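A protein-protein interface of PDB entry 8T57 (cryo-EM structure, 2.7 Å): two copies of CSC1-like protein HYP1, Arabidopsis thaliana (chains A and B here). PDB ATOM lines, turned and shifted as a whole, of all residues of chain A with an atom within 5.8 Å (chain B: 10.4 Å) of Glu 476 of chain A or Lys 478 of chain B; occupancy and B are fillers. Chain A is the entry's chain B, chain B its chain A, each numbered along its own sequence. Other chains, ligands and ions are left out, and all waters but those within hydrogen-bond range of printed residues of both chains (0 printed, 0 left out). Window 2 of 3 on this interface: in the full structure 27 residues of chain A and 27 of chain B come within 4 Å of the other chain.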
ATOM      1  N   ASN A 472     -16.474  35.961  20.676  1.00  0.00           N
ATOM      2  CA  ASN A 472     -15.497  35.704  19.641  1.00  0.00           C
ATOM      3  C   ASN A 472     -14.140  36.291  19.977  1.00  0.00           C
ATOM      4  O   ASN A 472     -13.117  35.690  19.670  1.00  0.00           O
ATOM      5  CB  ASN A 472     -15.982  36.223  18.319  1.00  0.00           C
ATOM      6  CG  ASN A 472     -17.069  35.376  17.741  1.00  0.00           C
ATOM      7  OD1 ASN A 472     -17.268  34.216  18.121  1.00  0.00           O
ATOM      8  ND2 ASN A 472     -17.780  35.927  16.800  1.00  0.00           N
ATOM      9  N   VAL A 473     -14.101  37.406  20.688  1.00  0.00           N
ATOM     10  CA  VAL A 473     -12.828  38.006  21.074  1.00  0.00           C
ATOM     11  C   VAL A 473     -12.021  37.041  21.911  1.00  0.00           C
ATOM     12  O   VAL A 473     -10.811  36.907  21.736  1.00  0.00           O
ATOM     13  CB  VAL A 473     -13.008  39.317  21.874  1.00  0.00           C
ATOM     14  CG1 VAL A 473     -11.658  39.777  22.482  1.00  0.00           C
ATOM     15  CG2 VAL A 473     -13.533  40.415  20.955  1.00  0.00           C
ATOM     16  N   PHE A 474     -12.673  36.329  22.794  1.00  0.00           N
ATOM     17  CA  PHE A 474     -11.927  35.454  23.662  1.00  0.00           C
ATOM     18  C   PHE A 474     -11.625  34.097  23.067  1.00  0.00           C
ATOM     19  O   PHE A 474     -11.059  33.237  23.739  1.00  0.00           O
ATOM     20  CB  PHE A 474     -12.658  35.278  24.950  1.00  0.00           C
ATOM     21  CG  PHE A 474     -12.711  36.496  25.674  1.00  0.00           C
ATOM     22  CD1 PHE A 474     -13.871  37.171  25.729  1.00  0.00           C
ATOM     23  CD2 PHE A 474     -11.601  37.014  26.280  1.00  0.00           C
ATOM     24  CE1 PHE A 474     -13.949  38.345  26.361  1.00  0.00           C
ATOM     25  CE2 PHE A 474     -11.675  38.195  26.921  1.00  0.00           C
ATOM     26  CZ  PHE A 474     -12.852  38.853  26.955  1.00  0.00           C
ATOM     27  N   LEU A 475     -11.977  33.889  21.806  1.00  0.00           N
ATOM     28  CA  LEU A 475     -11.664  32.644  21.135  1.00  0.00           C
ATOM     29  C   LEU A 475     -10.386  32.785  20.335  1.00  0.00           C
ATOM     30  O   LEU A 475      -9.954  31.835  19.689  1.00  0.00           O
ATOM     31  CB  LEU A 475     -12.794  32.192  20.209  1.00  0.00           C
ATOM     32  CG  LEU A 475     -14.144  31.878  20.869  1.00  0.00           C
ATOM     33  CD1 LEU A 475     -15.156  31.557  19.793  1.00  0.00           C
ATOM     34  CD2 LEU A 475     -14.015  30.717  21.828  1.00  0.00           C
ATOM     35  N   GLU A 476      -9.753  33.953  20.380  1.00  0.00           N
ATOM     36  CA  GLU A 476      -8.522  34.149  19.635  1.00  0.00           C
ATOM     37  C   GLU A 476      -7.413  34.697  20.520  1.00  0.00           C
ATOM     38  O   GLU A 476      -7.099  35.876  20.409  1.00  0.00           O
ATOM     39  CB  GLU A 476      -8.758  35.128  18.500  1.00  0.00           C
ATOM     40  CG  GLU A 476      -9.764  34.686  17.491  1.00  0.00           C
ATOM     41  CD  GLU A 476      -9.911  35.663  16.367  1.00  0.00           C
ATOM     42  OE1 GLU A 476      -8.921  36.016  15.784  1.00  0.00           O
ATOM     43  OE2 GLU A 476     -11.027  36.017  16.039  1.00  0.00           O
ATOM     44  N   PRO A 477      -6.787  33.889  21.389  1.00  0.00           N
ATOM     45  CA  PRO A 477      -5.819  34.303  22.382  1.00  0.00           C
ATOM     46  C   PRO A 477      -4.660  35.147  21.880  1.00  0.00           C
ATOM     47  O   PRO A 477      -4.206  36.048  22.577  1.00  0.00           O
ATOM     48  CB  PRO A 477      -5.299  32.965  22.893  1.00  0.00           C
ATOM     49  CG  PRO A 477      -6.434  32.028  22.698  1.00  0.00           C
ATOM     50  CD  PRO A 477      -7.049  32.447  21.399  1.00  0.00           C
ATOM     51  N   LYS A 478      -4.212  34.938  20.654  1.00  0.00           N
ATOM     52  CA  LYS A 478      -3.069  35.695  20.164  1.00  0.00           C
ATOM     53  C   LYS A 478      -3.371  37.168  19.950  1.00  0.00           C
ATOM     54  O   LYS A 478      -2.454  37.964  19.761  1.00  0.00           O
ATOM     55  CB  LYS A 478      -2.509  35.087  18.882  1.00  0.00           C
ATOM     56  CG  LYS A 478      -3.369  35.250  17.653  1.00  0.00           C
ATOM     57  CD  LYS A 478      -2.741  34.568  16.442  1.00  0.00           C
ATOM     58  CE  LYS A 478      -3.560  34.821  15.179  1.00  0.00           C
ATOM     59  NZ  LYS A 478      -2.969  34.151  13.986  1.00  0.00           N
ATOM     60  N   THR A 479      -4.647  37.542  19.901  1.00  0.00           N
ATOM     61  CA  THR A 479      -4.981  38.931  19.679  1.00  0.00           C
ATOM     62  C   THR A 479      -5.490  39.569  20.950  1.00  0.00           C
ATOM     63  O   THR A 479      -5.672  40.790  20.993  1.00  0.00           O
ATOM     64  CB  THR A 479      -6.063  39.117  18.606  1.00  0.00           C
ATOM     65  OG1 THR A 479      -7.271  38.525  19.039  1.00  0.00           O
ATOM     66  CG2 THR A 479      -5.642  38.441  17.354  1.00  0.00           C
ATOM     67  N   ILE A 480      -5.663  38.800  22.031  1.00  0.00           N
ATOM     68  CA  ILE A 480      -6.259  39.411  23.192  1.00  0.00           C
ATOM     69  C   ILE A 480      -5.436  40.567  23.695  1.00  0.00           C
ATOM     70  O   ILE A 480      -6.003  41.619  23.974  1.00  0.00           O
ATOM     71  CB  ILE A 480      -6.598  38.439  24.341  1.00  0.00           C
ATOM     72  CG1 ILE A 480      -7.743  37.527  23.905  1.00  0.00           C
ATOM     73  CG2 ILE A 480      -6.946  39.228  25.601  1.00  0.00           C
ATOM     74  CD1 ILE A 480      -8.016  36.361  24.843  1.00  0.00           C
ATOM     75  N   ASN B 472       1.448  27.704  15.782  1.00  0.00           N
ATOM     76  CA  ASN B 472       0.477  28.742  15.519  1.00  0.00           C
ATOM     77  C   ASN B 472      -0.880  28.177  15.147  1.00  0.00           C
ATOM     78  O   ASN B 472      -1.904  28.733  15.528  1.00  0.00           O
ATOM     79  CB  ASN B 472       0.973  29.668  14.447  1.00  0.00           C
ATOM     80  CG  ASN B 472       2.061  30.569  14.934  1.00  0.00           C
ATOM     81  OD1 ASN B 472       2.253  30.774  16.139  1.00  0.00           O
ATOM     82  ND2 ASN B 472       2.781  31.142  14.013  1.00  0.00           N
ATOM     83  N   VAL B 473      -0.919  27.028  14.492  1.00  0.00           N
ATOM     84  CA  VAL B 473      -2.193  26.412  14.132  1.00  0.00           C
ATOM     85  C   VAL B 473      -3.009  26.126  15.370  1.00  0.00           C
ATOM     86  O   VAL B 473      -4.218  26.348  15.399  1.00  0.00           O
ATOM     87  CB  VAL B 473      -2.012  25.092  13.347  1.00  0.00           C
ATOM     88  CG1 VAL B 473      -3.365  24.347  13.214  1.00  0.00           C
ATOM     89  CG2 VAL B 473      -1.475  25.391  11.951  1.00  0.00           C
ATOM     90  N   PHE B 474      -2.367  25.674  16.417  1.00  0.00           N
ATOM     91  CA  PHE B 474      -3.122  25.318  17.590  1.00  0.00           C
ATOM     92  C   PHE B 474      -3.426  26.479  18.511  1.00  0.00           C
ATOM     93  O   PHE B 474      -4.000  26.287  19.581  1.00  0.00           O
ATOM     94  CB  PHE B 474      -2.401  24.258  18.352  1.00  0.00           C
ATOM     95  CG  PHE B 474      -2.348  23.048  17.613  1.00  0.00           C
ATOM     96  CD1 PHE B 474      -1.186  22.680  17.049  1.00  0.00           C
ATOM     97  CD2 PHE B 474      -3.460  22.276  17.429  1.00  0.00           C
ATOM     98  CE1 PHE B 474      -1.108  21.573  16.306  1.00  0.00           C
ATOM     99  CE2 PHE B 474      -3.386  21.157  16.684  1.00  0.00           C
ATOM    100  CZ  PHE B 474      -2.206  20.816  16.126  1.00  0.00           C
ATOM    101  N   LEU B 475      -3.066  27.690  18.109  1.00  0.00           N
ATOM    102  CA  LEU B 475      -3.380  28.865  18.896  1.00  0.00           C
ATOM    103  C   LEU B 475      -4.651  29.512  18.388  1.00  0.00           C
ATOM    104  O   LEU B 475      -5.083  30.528  18.924  1.00  0.00           O
ATOM    105  CB  LEU B 475      -2.245  29.889  18.872  1.00  0.00           C
ATOM    106  CG  LEU B 475      -0.901  29.447  19.466  1.00  0.00           C
ATOM    107  CD1 LEU B 475       0.117  30.544  19.256  1.00  0.00           C
ATOM    108  CD2 LEU B 475      -1.042  29.141  20.939  1.00  0.00           C
ATOM    109  N   GLU B 476      -5.280  28.931  17.371  1.00  0.00           N
ATOM    110  CA  GLU B 476      -6.504  29.503  16.843  1.00  0.00           C
ATOM    111  C   GLU B 476      -7.618  28.469  16.762  1.00  0.00           C
ATOM    112  O   GLU B 476      -7.926  28.019  15.666  1.00  0.00           O
ATOM    113  CB  GLU B 476      -6.257  30.049  15.448  1.00  0.00           C
ATOM    114  CG  GLU B 476      -5.245  31.144  15.377  1.00  0.00           C
ATOM    115  CD  GLU B 476      -5.087  31.681  13.989  1.00  0.00           C
ATOM    116  OE1 GLU B 476      -6.070  32.038  13.397  1.00  0.00           O
ATOM    117  OE2 GLU B 476      -3.966  31.803  13.530  1.00  0.00           O
ATOM    118  N   PRO B 477      -8.253  28.080  17.878  1.00  0.00           N
ATOM    119  CA  PRO B 477      -9.227  27.013  17.968  1.00  0.00           C
ATOM    120  C   PRO B 477     -10.379  27.068  16.979  1.00  0.00           C
ATOM    121  O   PRO B 477     -10.833  26.034  16.504  1.00  0.00           O
ATOM    122  CB  PRO B 477      -9.756  27.187  19.387  1.00  0.00           C
ATOM    123  CG  PRO B 477      -8.623  27.792  20.132  1.00  0.00           C
ATOM    124  CD  PRO B 477      -7.998  28.744  19.160  1.00  0.00           C
ATOM    125  N   LYS B 478     -10.818  28.252  16.589  1.00  0.00           N
ATOM    126  CA  LYS B 478     -11.954  28.337  15.683  1.00  0.00           C
ATOM    127  C   LYS B 478     -11.645  27.839  14.282  1.00  0.00           C
ATOM    128  O   LYS B 478     -12.556  27.639  13.483  1.00  0.00           O
ATOM    129  CB  LYS B 478     -12.507  29.757  15.619  1.00  0.00           C
ATOM    130  CG  LYS B 478     -11.639  30.765  14.907  1.00  0.00           C
ATOM    131  CD  LYS B 478     -12.261  32.157  14.942  1.00  0.00           C
ATOM    132  CE  LYS B 478     -11.432  33.152  14.135  1.00  0.00           C
ATOM    133  NZ  LYS B 478     -12.017  34.523  14.166  1.00  0.00           N
ATOM    134  N   THR B 479     -10.367  27.702  13.937  1.00  0.00           N
ATOM    135  CA  THR B 479     -10.025  27.249  12.608  1.00  0.00           C
ATOM    136  C   THR B 479      -9.522  25.825  12.640  1.00  0.00           C
ATOM    137  O   THR B 479      -9.335  25.217  11.581  1.00  0.00           O
ATOM    138  CB  THR B 479      -8.935  28.107  11.950  1.00  0.00           C
ATOM    139  OG1 THR B 479      -7.733  27.995  12.685  1.00  0.00           O
ATOM    140  CG2 THR B 479      -9.350  29.530  11.962  1.00  0.00           C
ATOM    141  N   ILE B 480      -9.361  25.227  13.825  1.00  0.00           N
ATOM    142  CA  ILE B 480      -8.770  23.912  13.831  1.00  0.00           C
ATOM    143  C   ILE B 480      -9.591  22.932  13.037  1.00  0.00           C
ATOM    144  O   ILE B 480      -9.022  22.192  12.241  1.00  0.00           O
ATOM    145  CB  ILE B 480      -8.443  23.348  15.228  1.00  0.00           C
ATOM    146  CG1 ILE B 480      -7.299  24.154  15.840  1.00  0.00           C
ATOM    147  CG2 ILE B 480      -8.101  21.863  15.121  1.00  0.00           C
ATOM    148  CD1 ILE B 480      -7.039  23.867  17.310  1.00  0.00           C
ATOM    149  N   PRO B 481     -10.917  22.848  13.188  1.00  0.00           N
ATOM    150  CA  PRO B 481     -11.709  21.916  12.459  1.00  0.00           C
ATOM    151  C   PRO B 481     -11.477  21.957  10.968  1.00  0.00           C
ATOM    152  O   PRO B 481     -11.496  20.908  10.339  1.00  0.00           O
ATOM    153  CB  PRO B 481     -13.123  22.379  12.790  1.00  0.00           C
ATOM    154  CG  PRO B 481     -13.010  23.003  14.136  1.00  0.00           C
ATOM    155  CD  PRO B 481     -11.703  23.700  14.111  1.00  0.00           C
ATOM    156  N   ARG B 482     -11.186  23.115  10.379  1.00  0.00           N
ATOM    157  CA  ARG B 482     -11.019  23.132   8.938  1.00  0.00           C
ATOM    158  C   ARG B 482      -9.608  22.837   8.544  1.00  0.00           C
ATOM    159  O   ARG B 482      -9.359  22.231   7.503  1.00  0.00           O
ATOM    160  CB  ARG B 482     -11.413  24.469   8.370  1.00  0.00           C
ATOM    161  CG  ARG B 482     -12.874  24.852   8.534  1.00  0.00           C
ATOM    162  CD  ARG B 482     -13.758  24.006   7.720  1.00  0.00           C
ATOM    163  NE  ARG B 482     -15.134  24.435   7.774  1.00  0.00           N
ATOM    164  CZ  ARG B 482     -15.692  25.357   6.958  1.00  0.00           C
ATOM    165  NH1 ARG B 482     -14.977  25.963   6.031  1.00  0.00           N
ATOM    166  NH2 ARG B 482     -16.969  25.664   7.095  1.00  0.00           N
ATOM    167  N   VAL B 483      -8.669  23.214   9.385  1.00  0.00           N
ATOM    168  CA  VAL B 483      -7.297  22.949   9.055  1.00  0.00           C
ATOM    169  C   VAL B 483      -7.092  21.449   9.033  1.00  0.00           C
ATOM    170  O   VAL B 483      -6.409  20.937   8.151  1.00  0.00           O
ATOM    171  CB  VAL B 483      -6.331  23.607  10.045  1.00  0.00           C
ATOM    172  CG1 VAL B 483      -4.934  23.143   9.765  1.00  0.00           C
ATOM    173  CG2 VAL B 483      -6.402  25.104   9.909  1.00  0.00           C
ATOM    174  N   LEU B 484      -7.658  20.737  10.008  1.00  0.00           N
ATOM    175  CA  LEU B 484      -7.497  19.300  10.015  1.00  0.00           C
ATOM    176  C   LEU B 484      -8.430  18.612   9.038  1.00  0.00           C
ATOM    177  O   LEU B 484      -8.020  17.718   8.309  1.00  0.00           O
ATOM    178  CB  LEU B 484      -7.758  18.746  11.392  1.00  0.00           C
ATOM    179  CG  LEU B 484      -6.819  19.164  12.464  1.00  0.00           C
ATOM    180  CD1 LEU B 484      -7.328  18.615  13.740  1.00  0.00           C
ATOM    181  CD2 LEU B 484      -5.417  18.669  12.193  1.00  0.00           C
ATOM    182  N   ALA B 485      -9.658  19.060   8.887  1.00  0.00           N
ATOM    183  CA  ALA B 485     -10.531  18.371   7.960  1.00  0.00           C
ATOM    184  C   ALA B 485      -9.987  18.395   6.552  1.00  0.00           C
ATOM    185  O   ALA B 485     -10.200  17.458   5.791  1.00  0.00           O
ATOM    186  CB  ALA B 485     -11.905  18.968   7.993  1.00  0.00           C
ATOM    187  N   ILE B 615     -13.927  16.476  15.887  1.00  0.00           N
ATOM    188  CA  ILE B 615     -13.520  17.810  15.460  1.00  0.00           C
ATOM    189  C   ILE B 615     -13.318  17.810  13.971  1.00  0.00           C
ATOM    190  O   ILE B 615     -13.770  18.724  13.279  1.00  0.00           O
ATOM    191  CB  ILE B 615     -12.232  18.280  16.178  1.00  0.00           C
ATOM    192  CG1 ILE B 615     -12.536  18.548  17.664  1.00  0.00           C
ATOM    193  CG2 ILE B 615     -11.607  19.483  15.479  1.00  0.00           C
ATOM    194  CD1 ILE B 615     -11.307  18.720  18.555  1.00  0.00           C
ATOM    195  N   VAL B 618     -16.691  17.669  12.268  1.00  0.00           N
ATOM    196  CA  VAL B 618     -17.389  18.932  12.255  1.00  0.00           C
ATOM    197  C   VAL B 618     -16.833  19.783  11.153  1.00  0.00           C
ATOM    198  O   VAL B 618     -17.588  20.391  10.383  1.00  0.00           O
ATOM    199  CB  VAL B 618     -17.220  19.653  13.593  1.00  0.00           C
ATOM    200  CG1 VAL B 618     -17.726  21.060  13.520  1.00  0.00           C
ATOM    201  CG2 VAL B 618     -18.011  18.938  14.634  1.00  0.00           C
ATOM    202  N   GLY B 619     -15.516  19.835  11.059  1.00  0.00           N
ATOM    203  CA  GLY B 619     -14.892  20.616  10.034  1.00  0.00           C
ATOM    204  C   GLY B 619     -15.221  20.102   8.657  1.00  0.00           C
ATOM    205  O   GLY B 619     -15.478  20.896   7.750  1.00  0.00           O
ATOM    206  N   SER B 630     -22.860  19.556  10.454  1.00  0.00           N
ATOM    207  CA  SER B 630     -21.722  20.155  11.124  1.00  0.00           C
ATOM    208  C   SER B 630     -22.158  20.644  12.487  1.00  0.00           C
ATOM    209  O   SER B 630     -21.496  20.378  13.491  1.00  0.00           O
ATOM    210  CB  SER B 630     -21.176  21.289  10.306  1.00  0.00           C
ATOM    211  OG  SER B 630     -20.076  21.869  10.920  1.00  0.00           O
ATOM    212  N   ILE B 634     -21.804  19.006  16.890  1.00  0.00           N
ATOM    213  CA  ILE B 634     -21.136  19.671  18.015  1.00  0.00           C
ATOM    214  C   ILE B 634     -21.418  18.966  19.352  1.00  0.00           C
ATOM    215  O   ILE B 634     -20.511  18.867  20.181  1.00  0.00           O
ATOM    216  CB  ILE B 634     -21.439  21.184  18.106  1.00  0.00           C
ATOM    217  CG1 ILE B 634     -20.871  21.949  16.907  1.00  0.00           C
ATOM    218  CG2 ILE B 634     -20.901  21.725  19.433  1.00  0.00           C
ATOM    219  CD1 ILE B 634     -19.394  22.002  16.780  1.00  0.00           C
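Leu 475 of chain A touches one residue of chain B. Of chain B, only Leu 475 (3.7 Å) comes within 4 Å of Pro 477 of chain A. Of the printed residues of chain B, Lys 478 of chain A touches Glu 476 (2.6 Å). No residue of chain B comes within 4 Å of Thr 479 of chain A. Phe 474 of chain B touches none of the printed residues of chain A. Printed residues of chain A within 4 Å of Leu 475 of chain B: Pro 477. Printed residues of chain A within 4 Å of Glu 476 of chain B: Lys 478 (2.6 Å). Of the printed residues of chain A, Pro 477 of chain B touches Leu 475. Lys 478 of chain B touches just one residue of chain A: Glu 476. Ile 634 of chain B touches none of the printed residues of chain A. The nearest residue of chain A that does not touch Lys 478 of chain B is Leu 475 of chain A (4.8 Å).
Leu 475 of chain A touches Pro 477 of chain B, and with the chains exchanged Pro 477 of chain A touches Leu 475 of chain B. Glu 476 of chain A touches Lys 478 of chain B, and with the chains exchanged Lys 478 of chain A touches Glu 476 of chain B. 9 positions are printed for both chains.
Pro 477 of chain B touches Leu 475 of chain A (CD to O, 3.7 Å). O of Leu 475 of chain B touches CD of Pro 477 of chain A, at 3.7 Å.
The backbone carbonyl oxygen (O) of Glu 476 of chain B sits at hydrogen-bond distance from the side-chain hydroxyl (OG1) of Thr 479 of chain B (3.0 Å). The backbone carbonyl oxygen (O) of Glu 476 of chain A lies within hydrogen-bond range of the side-chain hydroxyl (OG1) of Thr 479 of chain A.
The side-chain amino group (NZ) of Lys 478 of chain B lies within salt-bridge range of the side-chain carboxylate (OE2) of Glu 476 of chain A (2.6 Å). The side-chain carboxylate of Glu 476 of chain B lies within salt-bridge range of the side-chain amino group of Lys 478 of chain A (2.6 Å).
Of the 19 printed residues of chain B, 4 touch a printed residue of chain A. Hydrophobic or aromatic side chains of chain B within 4 Å of the printed part of chain A: Pro 477. Among the printed residues, 4 pairs touch across the chains.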
